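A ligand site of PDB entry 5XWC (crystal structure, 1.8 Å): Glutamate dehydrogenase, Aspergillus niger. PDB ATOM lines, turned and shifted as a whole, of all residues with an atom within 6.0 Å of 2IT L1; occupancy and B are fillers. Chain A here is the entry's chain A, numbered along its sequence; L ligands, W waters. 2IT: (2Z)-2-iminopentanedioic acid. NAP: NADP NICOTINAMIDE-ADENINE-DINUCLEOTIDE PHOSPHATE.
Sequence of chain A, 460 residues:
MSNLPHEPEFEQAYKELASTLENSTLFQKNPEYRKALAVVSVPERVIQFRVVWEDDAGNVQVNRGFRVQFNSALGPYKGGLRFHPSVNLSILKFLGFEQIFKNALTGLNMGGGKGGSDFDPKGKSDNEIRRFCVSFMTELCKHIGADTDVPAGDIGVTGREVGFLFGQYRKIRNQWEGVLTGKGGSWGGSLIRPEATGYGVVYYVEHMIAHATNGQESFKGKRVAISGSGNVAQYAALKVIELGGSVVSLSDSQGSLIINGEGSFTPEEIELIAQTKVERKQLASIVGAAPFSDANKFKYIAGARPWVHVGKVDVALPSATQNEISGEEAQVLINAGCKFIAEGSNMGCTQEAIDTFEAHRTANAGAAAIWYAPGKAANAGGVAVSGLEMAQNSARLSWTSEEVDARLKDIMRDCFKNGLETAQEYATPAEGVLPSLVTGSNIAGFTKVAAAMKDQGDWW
Water W1 lies within hydrogen-bond range of O of Asn 379, N of Val 383, OAE of 2IT L1 and N of Gly 382.
OD1 of Asn 346 lies within hydrogen-bond range of NZ of Lys 102 (2.8 Å). The backbone carbonyl oxygen of Gly 382 sits at hydrogen-bond distance from the guanidinium group of Arg 193 (3.1 Å). The side-chain amide oxygen of Asn 346 lies within hydrogen-bond range of the side-chain amide nitrogen of Asn 379 (3.3 Å). ND2 of Asn 103 is in hydrogen-bond range of O of Lys 78. NZ of Lys 114 is in hydrogen-bond range of OE1 of Gln 99 (3.4 Å). NZ of Lys 102 lies within hydrogen-bond range of OD1 of Asn 379 (2.8 Å). The side-chain amide nitrogen of Gln 99 is in hydrogen-bond range of the side-chain amide oxygen of Asn 103. The backbone NH (N) of Gly 382 lies close to the side-chain hydroxyl (OG1) of Thr 197.
An oxygen (O7N) of NAP L2 is in hydrogen-bond range of the guanidinium group (NH2) of Arg 193 (2.8 Å). An oxygen (OAE) of 2IT L1 lies within hydrogen-bond range of the side-chain amide nitrogen (NE2) of Gln 99 (3.1 Å). The backbone NH of Asn 346 lies within hydrogen-bond range of an oxygen (O3D) of NAP L2, 3.1 Å away. The guanidinium group of Arg 193 lies within salt-bridge range of an oxygen (OAD) of 2IT L1 (2.9 Å). The backbone carbonyl oxygen of Gly 153 is in hydrogen-bond range of a nitrogen (NAA) of 2IT L1, at 3.4 Å. The side-chain hydroxyl (OG) of Ser 386 lies within hydrogen-bond range of an oxygen (OAD) of 2IT L1. The side-chain amino group of Lys 78 is in salt-bridge range of an oxygen (OAB) of 2IT L1 (2.7 Å). NZ of Lys 102 lies within salt-bridge range of OAE of 2IT L1, at 2.7 Å. The side-chain amide nitrogen (ND2) of Asn 346 is in hydrogen-bond range of an oxygen (OAC) of 2IT L1 (2.8 Å). OD1 of Asp 154 is in hydrogen-bond range of NAA of 2IT L1, 3.0 Å away. OD1 of Asp 154 is in hydrogen-bond range of O2D of NAP L2, at 2.6 Å. The side-chain amino group (NZ) of Lys 114 lies within salt-bridge range of an oxygen (OAC) of 2IT L1. An oxygen (O7N) of NAP L2 sits at hydrogen-bond distance from the side-chain hydroxyl of Thr 197 (2.8 Å). The side-chain amide nitrogen (ND2) of Asn 346 is in hydrogen-bond range of an oxygen (O2D) of NAP L2, at 2.8 Å.
Gly 79 touches 2IT L1. N of Gly 80 touches CAF of 2IT L1 (3.6 Å). Ala 152 touches 2IT L1. Gly 382 touches 2IT L1. Val 383 touches 2IT L1. Hydrophobic or aromatic side chains within 4 Å of 2IT L1: Ala 152 and Val 383. Within 4 Å of 2IT L1: Lys 78, Gly 79, Gly 80, Gln 99, Lys 102, Lys 114, Ala 152, Gly 153, Asp 154, Arg 193, Asn 346, Gly 382, Val 383 and Ser 386. The nearest printed residue that does not touch 2IT L1 is Thr 181 (4.1 Å).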
ATOM      1  N   LYS A  78     -19.212 -26.625 -24.094  1.00  0.00           N
ATOM      2  CA  LYS A  78     -19.805 -25.677 -23.175  1.00  0.00           C
ATOM      3  C   LYS A  78     -21.000 -25.043 -23.887  1.00  0.00           C
ATOM      4  O   LYS A  78     -20.887 -24.606 -25.036  1.00  0.00           O
ATOM      5  CB  LYS A  78     -18.832 -24.554 -22.832  1.00  0.00           C
ATOM      6  CG  LYS A  78     -19.343 -23.611 -21.765  1.00  0.00           C
ATOM      7  CD  LYS A  78     -19.109 -24.138 -20.379  1.00  0.00           C
ATOM      8  CE  LYS A  78     -19.874 -23.340 -19.340  1.00  0.00           C
ATOM      9  NZ  LYS A  78     -21.332 -23.644 -19.267  1.00  0.00           N
ATOM     10  N   GLY A  79     -22.124 -25.046 -23.178  1.00  0.00           N
ATOM     11  CA  GLY A  79     -23.307 -24.344 -23.650  1.00  0.00           C
ATOM     12  C   GLY A  79     -24.533 -24.849 -22.947  1.00  0.00           C
ATOM     13  O   GLY A  79     -24.511 -25.899 -22.307  1.00  0.00           O
ATOM     14  N   GLY A  80     -25.614 -24.106 -23.075  1.00  0.00           N
ATOM     15  CA  GLY A  80     -26.805 -24.352 -22.293  1.00  0.00           C
ATOM     16  C   GLY A  80     -27.715 -25.495 -22.680  1.00  0.00           C
ATOM     17  O   GLY A  80     -27.489 -26.203 -23.673  1.00  0.00           O
ATOM     18  N   LEU A  95     -27.772 -23.824 -32.424  1.00  0.00           N
ATOM     19  CA  LEU A  95     -27.290 -23.238 -31.181  1.00  0.00           C
ATOM     20  C   LEU A  95     -25.863 -23.676 -30.821  1.00  0.00           C
ATOM     21  O   LEU A  95     -25.002 -22.852 -30.471  1.00  0.00           O
ATOM     22  CB  LEU A  95     -28.262 -23.575 -30.050  1.00  0.00           C
ATOM     23  CG  LEU A  95     -29.603 -22.831 -30.092  1.00  0.00           C
ATOM     24  CD1 LEU A  95     -30.656 -23.585 -29.312  1.00  0.00           C
ATOM     25  CD2 LEU A  95     -29.443 -21.391 -29.605  1.00  0.00           C
ATOM     26  N   GLN A  99     -22.464 -21.555 -30.736  1.00  0.00           N
ATOM     27  CA  GLN A  99     -21.719 -21.589 -29.484  1.00  0.00           C
ATOM     28  C   GLN A  99     -20.211 -21.765 -29.662  1.00  0.00           C
ATOM     29  O   GLN A  99     -19.426 -21.252 -28.842  1.00  0.00           O
ATOM     30  CB  GLN A  99     -22.269 -22.701 -28.560  1.00  0.00           C
ATOM     31  CG  GLN A  99     -21.943 -22.473 -27.098  1.00  0.00           C
ATOM     32  CD  GLN A  99     -22.844 -21.427 -26.455  1.00  0.00           C
ATOM     33  OE1 GLN A  99     -24.037 -21.427 -26.686  1.00  0.00           O
ATOM     34  NE2 GLN A  99     -22.280 -20.565 -25.631  1.00  0.00           N
ATOM     35  N   LYS A 102     -18.905 -18.205 -30.631  1.00  0.00           N
ATOM     36  CA  LYS A 102     -19.140 -17.350 -29.482  1.00  0.00           C
ATOM     37  C   LYS A 102     -18.112 -17.617 -28.401  1.00  0.00           C
ATOM     38  O   LYS A 102     -17.483 -16.700 -27.847  1.00  0.00           O
ATOM     39  CB  LYS A 102     -20.525 -17.595 -28.924  1.00  0.00           C
ATOM     40  CG  LYS A 102     -20.879 -16.747 -27.692  1.00  0.00           C
ATOM     41  CD  LYS A 102     -22.189 -17.186 -27.033  1.00  0.00           C
ATOM     42  CE  LYS A 102     -23.268 -17.509 -28.035  1.00  0.00           C
ATOM     43  NZ  LYS A 102     -24.572 -17.684 -27.373  1.00  0.00           N
ATOM     44  N   ASN A 103     -17.946 -18.900 -28.081  1.00  0.00           N
ATOM     45  CA  ASN A 103     -17.002 -19.243 -27.029  1.00  0.00           C
ATOM     46  C   ASN A 103     -15.571 -18.859 -27.370  1.00  0.00           C
ATOM     47  O   ASN A 103     -14.840 -18.385 -26.500  1.00  0.00           O
ATOM     48  CB  ASN A 103     -17.147 -20.743 -26.680  1.00  0.00           C
ATOM     49  CG  ASN A 103     -18.471 -21.030 -26.017  1.00  0.00           C
ATOM     50  OD1 ASN A 103     -19.328 -20.127 -25.870  1.00  0.00           O
ATOM     51  ND2 ASN A 103     -18.668 -22.266 -25.591  1.00  0.00           N
ATOM     52  N   LYS A 114     -24.631 -27.697 -27.038  1.00  0.00           N
ATOM     53  CA  LYS A 114     -25.971 -27.272 -26.626  1.00  0.00           C
ATOM     54  C   LYS A 114     -26.798 -28.537 -26.448  1.00  0.00           C
ATOM     55  O   LYS A 114     -26.571 -29.535 -27.155  1.00  0.00           O
ATOM     56  CB  LYS A 114     -26.638 -26.388 -27.688  1.00  0.00           C
ATOM     57  CG  LYS A 114     -27.632 -25.414 -27.078  1.00  0.00           C
ATOM     58  CD  LYS A 114     -26.902 -24.193 -26.534  1.00  0.00           C
ATOM     59  CE  LYS A 114     -27.898 -23.250 -25.885  1.00  0.00           C
ATOM     60  NZ  LYS A 114     -27.256 -21.925 -25.769  1.00  0.00           N
ATOM     61  N   VAL A 150     -19.826 -29.078 -19.976  1.00  0.00           N
ATOM     62  CA  VAL A 150     -20.338 -28.284 -18.864  1.00  0.00           C
ATOM     63  C   VAL A 150     -21.593 -27.524 -19.356  1.00  0.00           C
ATOM     64  O   VAL A 150     -21.460 -26.481 -19.971  1.00  0.00           O
ATOM     65  CB  VAL A 150     -19.280 -27.325 -18.284  1.00  0.00           C
ATOM     66  CG1 VAL A 150     -19.831 -26.485 -17.138  1.00  0.00           C
ATOM     67  CG2 VAL A 150     -18.067 -28.106 -17.789  1.00  0.00           C
ATOM     68  N   PRO A 151     -22.789 -28.081 -19.110  1.00  0.00           N
ATOM     69  CA  PRO A 151     -23.989 -27.342 -19.487  1.00  0.00           C
ATOM     70  C   PRO A 151     -24.351 -26.197 -18.512  1.00  0.00           C
ATOM     71  O   PRO A 151     -23.585 -25.823 -17.620  1.00  0.00           O
ATOM     72  CB  PRO A 151     -25.059 -28.418 -19.549  1.00  0.00           C
ATOM     73  CG  PRO A 151     -24.297 -29.734 -19.591  1.00  0.00           C
ATOM     74  CD  PRO A 151     -23.147 -29.455 -18.717  1.00  0.00           C
ATOM     75  N   ALA A 152     -25.509 -25.603 -18.773  1.00  0.00           N
ATOM     76  CA  ALA A 152     -26.010 -24.447 -18.042  1.00  0.00           C
ATOM     77  C   ALA A 152     -27.465 -24.282 -18.479  1.00  0.00           C
ATOM     78  O   ALA A 152     -28.021 -25.171 -19.153  1.00  0.00           O
ATOM     79  CB  ALA A 152     -25.200 -23.202 -18.389  1.00  0.00           C
ATOM     80  N   GLY A 153     -28.061 -23.164 -18.110  1.00  0.00           N
ATOM     81  CA  GLY A 153     -29.411 -22.828 -18.540  1.00  0.00           C
ATOM     82  C   GLY A 153     -29.443 -22.248 -19.941  1.00  0.00           C
ATOM     83  O   GLY A 153     -28.409 -22.136 -20.594  1.00  0.00           O
ATOM     84  N   ASP A 154     -30.655 -21.922 -20.364  1.00  0.00           N
ATOM     85  CA  ASP A 154     -31.025 -21.315 -21.652  1.00  0.00           C
ATOM     86  C   ASP A 154     -32.544 -21.172 -21.546  1.00  0.00           C
ATOM     87  O   ASP A 154     -33.063 -21.101 -20.430  1.00  0.00           O
ATOM     88  CB  ASP A 154     -30.589 -22.137 -22.871  1.00  0.00           C
ATOM     89  CG  ASP A 154     -30.624 -21.341 -24.192  1.00  0.00           C
ATOM     90  OD1 ASP A 154     -29.695 -20.538 -24.475  1.00  0.00           O
ATOM     91  OD2 ASP A 154     -31.593 -21.555 -24.968  1.00  0.00           O
ATOM     92  N   THR A 181     -22.917 -24.795 -14.930  1.00  0.00           N
ATOM     93  CA  THR A 181     -22.833 -23.426 -14.458  1.00  0.00           C
ATOM     94  C   THR A 181     -24.246 -22.837 -14.386  1.00  0.00           C
ATOM     95  O   THR A 181     -25.235 -23.518 -14.733  1.00  0.00           O
ATOM     96  CB  THR A 181     -21.892 -22.583 -15.345  1.00  0.00           C
ATOM     97  OG1 THR A 181     -22.345 -22.593 -16.719  1.00  0.00           O
ATOM     98  CG2 THR A 181     -20.506 -23.137 -15.261  1.00  0.00           C
ATOM     99  N   ARG A 193     -23.282 -14.112 -12.491  1.00  0.00           N
ATOM    100  CA  ARG A 193     -23.797 -15.011 -13.538  1.00  0.00           C
ATOM    101  C   ARG A 193     -25.266 -14.732 -13.944  1.00  0.00           C
ATOM    102  O   ARG A 193     -25.572 -14.743 -15.124  1.00  0.00           O
ATOM    103  CB  ARG A 193     -23.594 -16.519 -13.210  1.00  0.00           C
ATOM    104  CG  ARG A 193     -24.043 -17.447 -14.354  1.00  0.00           C
ATOM    105  CD  ARG A 193     -23.224 -17.227 -15.622  1.00  0.00           C
ATOM    106  NE  ARG A 193     -23.730 -17.909 -16.832  1.00  0.00           N
ATOM    107  CZ  ARG A 193     -24.695 -17.490 -17.635  1.00  0.00           C
ATOM    108  NH1 ARG A 193     -25.414 -16.383 -17.345  1.00  0.00           N
ATOM    109  NH2 ARG A 193     -25.005 -18.171 -18.728  1.00  0.00           N
ATOM    110  N   THR A 197     -25.389 -12.171 -19.087  1.00  0.00           N
ATOM    111  CA  THR A 197     -25.694 -12.094 -20.513  1.00  0.00           C
ATOM    112  C   THR A 197     -26.256 -10.702 -20.860  1.00  0.00           C
ATOM    113  O   THR A 197     -25.759 -10.035 -21.774  1.00  0.00           O
ATOM    114  CB  THR A 197     -26.631 -13.191 -20.969  1.00  0.00           C
ATOM    115  OG1 THR A 197     -26.034 -14.472 -20.638  1.00  0.00           O
ATOM    116  CG2 THR A 197     -26.809 -13.125 -22.457  1.00  0.00           C
ATOM    117  N   ASN A 346     -30.012 -15.864 -29.307  1.00  0.00           N
ATOM    118  CA  ASN A 346     -29.245 -16.525 -30.339  1.00  0.00           C
ATOM    119  C   ASN A 346     -30.022 -16.519 -31.661  1.00  0.00           C
ATOM    120  O   ASN A 346     -31.174 -16.955 -31.716  1.00  0.00           O
ATOM    121  CB  ASN A 346     -28.903 -17.959 -29.908  1.00  0.00           C
ATOM    122  CG  ASN A 346     -27.820 -17.970 -28.848  1.00  0.00           C
ATOM    123  OD1 ASN A 346     -26.735 -17.468 -29.090  1.00  0.00           O
ATOM    124  ND2 ASN A 346     -28.135 -18.475 -27.664  1.00  0.00           N
ATOM    125  N   ASN A 379     -23.884 -11.420 -26.976  1.00  0.00           N
ATOM    126  CA  ASN A 379     -24.471 -12.208 -25.886  1.00  0.00           C
ATOM    127  C   ASN A 379     -23.463 -13.167 -25.199  1.00  0.00           C
ATOM    128  O   ASN A 379     -23.857 -13.877 -24.274  1.00  0.00           O
ATOM    129  CB  ASN A 379     -25.781 -12.879 -26.298  1.00  0.00           C
ATOM    130  CG  ASN A 379     -25.610 -14.143 -27.124  1.00  0.00           C
ATOM    131  OD1 ASN A 379     -24.644 -14.908 -26.944  1.00  0.00           O
ATOM    132  ND2 ASN A 379     -26.559 -14.372 -28.045  1.00  0.00           N
ATOM    133  N   ALA A 380     -22.194 -13.062 -25.561  1.00  0.00           N
ATOM    134  CA  ALA A 380     -21.105 -13.922 -25.079  1.00  0.00           C
ATOM    135  C   ALA A 380     -20.762 -13.741 -23.617  1.00  0.00           C
ATOM    136  O   ALA A 380     -20.009 -14.525 -23.047  1.00  0.00           O
ATOM    137  CB  ALA A 380     -19.863 -13.669 -25.905  1.00  0.00           C
ATOM    138  N   GLY A 382     -22.595 -14.197 -21.048  1.00  0.00           N
ATOM    139  CA  GLY A 382     -23.184 -15.247 -20.207  1.00  0.00           C
ATOM    140  C   GLY A 382     -22.224 -16.417 -20.113  1.00  0.00           C
ATOM    141  O   GLY A 382     -21.818 -16.828 -19.024  1.00  0.00           O
ATOM    142  N   VAL A 383     -21.867 -16.942 -21.271  1.00  0.00           N
ATOM    143  CA  VAL A 383     -20.937 -18.080 -21.324  1.00  0.00           C
ATOM    144  C   VAL A 383     -19.553 -17.688 -20.768  1.00  0.00           C
ATOM    145  O   VAL A 383     -18.845 -18.517 -20.178  1.00  0.00           O
ATOM    146  CB  VAL A 383     -20.891 -18.728 -22.721  1.00  0.00           C
ATOM    147  CG1 VAL A 383     -20.088 -17.914 -23.727  1.00  0.00           C
ATOM    148  CG2 VAL A 383     -20.276 -20.156 -22.606  1.00  0.00           C
ATOM    149  N   ALA A 384     -19.141 -16.426 -20.972  1.00  0.00           N
ATOM    150  CA  ALA A 384     -17.897 -15.936 -20.392  1.00  0.00           C
ATOM    151  C   ALA A 384     -17.922 -16.046 -18.878  1.00  0.00           C
ATOM    152  O   ALA A 384     -16.970 -16.595 -18.279  1.00  0.00           O
ATOM    153  CB  ALA A 384     -17.589 -14.495 -20.827  1.00  0.00           C
ATOM    154  N   SER A 386     -19.955 -17.961 -17.169  1.00  0.00           N
ATOM    155  CA  SER A 386     -19.933 -19.414 -16.902  1.00  0.00           C
ATOM    156  C   SER A 386     -18.497 -19.953 -16.853  1.00  0.00           C
ATOM    157  O   SER A 386     -18.153 -20.724 -15.971  1.00  0.00           O
ATOM    158  CB  SER A 386     -20.726 -20.199 -17.963  1.00  0.00           C
ATOM    159  OG  SER A 386     -22.114 -20.182 -17.749  1.00  0.00           O
HETATM  160  OAC 2IT L   1     -26.517 -19.218 -25.444  1.00  0.00           O
HETATM  161  CAJ 2IT L   1     -25.687 -19.002 -24.548  1.00  0.00           C
HETATM  162  OAE 2IT L   1     -24.525 -18.572 -24.801  1.00  0.00           O
HETATM  163  CAI 2IT L   1     -26.089 -19.379 -23.165  1.00  0.00           C
HETATM  164  NAA 2IT L   1     -27.317 -19.869 -22.847  1.00  0.00           N
HETATM  165  CAG 2IT L   1     -25.048 -19.464 -22.056  1.00  0.00           C
HETATM  166  CAF 2IT L   1     -24.583 -20.886 -21.920  1.00  0.00           C
HETATM  167  CAH 2IT L   1     -23.542 -21.132 -20.853  1.00  0.00           C
HETATM  168  OAB 2IT L   1     -22.864 -22.194 -20.969  1.00  0.00           O
HETATM  169  OAD 2IT L   1     -23.418 -20.332 -19.911  1.00  0.00           O
HETATM  170  PA  NAP L   2     -35.693 -17.498 -20.553  1.00  0.00           P
HETATM  171  O1A NAP L   2     -35.348 -16.881 -19.229  1.00  0.00           O
HETATM  172  O2A NAP L   2     -36.455 -18.748 -20.661  1.00  0.00           O
HETATM  173  O5B NAP L   2     -36.612 -16.406 -21.329  1.00  0.00           O
HETATM  174  C5B NAP L   2     -36.987 -16.604 -22.677  1.00  0.00           C
HETATM  175  C4B NAP L   2     -37.964 -15.458 -23.016  1.00  0.00           C
HETATM  176  O4B NAP L   2     -38.206 -15.522 -24.416  1.00  0.00           O
HETATM  177  C3B NAP L   2     -39.311 -15.551 -22.338  1.00  0.00           C
HETATM  178  O3B NAP L   2     -39.872 -14.220 -22.145  1.00  0.00           O
HETATM  179  C2B NAP L   2     -40.090 -16.373 -23.345  1.00  0.00           C
HETATM  180  O2B NAP L   2     -41.510 -16.250 -23.323  1.00  0.00           O
HETATM  181  C1B NAP L   2     -39.561 -15.897 -24.668  1.00  0.00           C
HETATM  182  N9A NAP L   2     -39.639 -16.972 -25.681  1.00  0.00           N
HETATM  183  C8A NAP L   2     -38.961 -18.158 -25.630  1.00  0.00           C
HETATM  184  N7A NAP L   2     -39.248 -18.922 -26.714  1.00  0.00           N
HETATM  185  C5A NAP L   2     -40.109 -18.217 -27.453  1.00  0.00           C
HETATM  186  C6A NAP L   2     -40.798 -18.472 -28.720  1.00  0.00           C
HETATM  187  N6A NAP L   2     -40.567 -19.638 -29.350  1.00  0.00           N
HETATM  188  N1A NAP L   2     -41.615 -17.500 -29.194  1.00  0.00           N
HETATM  189  C2A NAP L   2     -41.793 -16.337 -28.524  1.00  0.00           C
HETATM  190  N3A NAP L   2     -41.190 -16.044 -27.359  1.00  0.00           N
HETATM  191  C4A NAP L   2     -40.359 -16.947 -26.785  1.00  0.00           C
HETATM  192  O3  NAP L   2     -34.424 -17.573 -21.518  1.00  0.00           O
HETATM  193  PN  NAP L   2     -33.118 -16.643 -21.622  1.00  0.00           P
HETATM  194  O1N NAP L   2     -33.492 -15.239 -21.242  1.00  0.00           O
HETATM  195  O2N NAP L   2     -31.983 -17.306 -20.895  1.00  0.00           O
HETATM  196  O5D NAP L   2     -32.832 -16.769 -23.176  1.00  0.00           O
HETATM  197  C5D NAP L   2     -33.256 -15.765 -24.133  1.00  0.00           C
HETATM  198  C4D NAP L   2     -32.400 -15.786 -25.374  1.00  0.00           C
HETATM  199  O4D NAP L   2     -31.055 -15.465 -25.014  1.00  0.00           O
HETATM  200  C3D NAP L   2     -32.326 -17.154 -26.088  1.00  0.00           C
HETATM  201  O3D NAP L   2     -32.200 -16.971 -27.490  1.00  0.00           O
HETATM  202  C2D NAP L   2     -31.058 -17.768 -25.508  1.00  0.00           C
HETATM  203  O2D NAP L   2     -30.526 -18.871 -26.275  1.00  0.00           O
HETATM  204  C1D NAP L   2     -30.184 -16.522 -25.477  1.00  0.00           C
HETATM  205  N1N NAP L   2     -28.993 -16.563 -24.607  1.00  0.00           N
HETATM  206  C2N NAP L   2     -29.110 -16.883 -23.315  1.00  0.00           C
HETATM  207  C3N NAP L   2     -27.994 -16.907 -22.471  1.00  0.00           C
HETATM  208  C7N NAP L   2     -28.094 -17.176 -21.005  1.00  0.00           C
HETATM  209  O7N NAP L   2     -27.064 -17.032 -20.322  1.00  0.00           O
HETATM  210  N7N NAP L   2     -29.289 -17.380 -20.402  1.00  0.00           N
HETATM  211  C4N NAP L   2     -26.747 -16.572 -23.016  1.00  0.00           C
HETATM  212  C5N NAP L   2     -26.662 -16.200 -24.357  1.00  0.00           C
HETATM  213  C6N NAP L   2     -27.800 -16.174 -25.133  1.00  0.00           C
HETATM  214  P2B NAP L   2     -42.456 -16.979 -22.231  1.00  0.00           P
HETATM  215  O1X NAP L   2     -42.116 -16.146 -20.957  1.00  0.00           O
HETATM  216  O2X NAP L   2     -42.085 -18.316 -21.884  1.00  0.00           O
HETATM  217  O3X NAP L   2     -43.828 -16.858 -22.900  1.00  0.00           O
HETATM  218  O   HOH W   1     -23.281 -16.405 -23.592  1.00  0.00           O
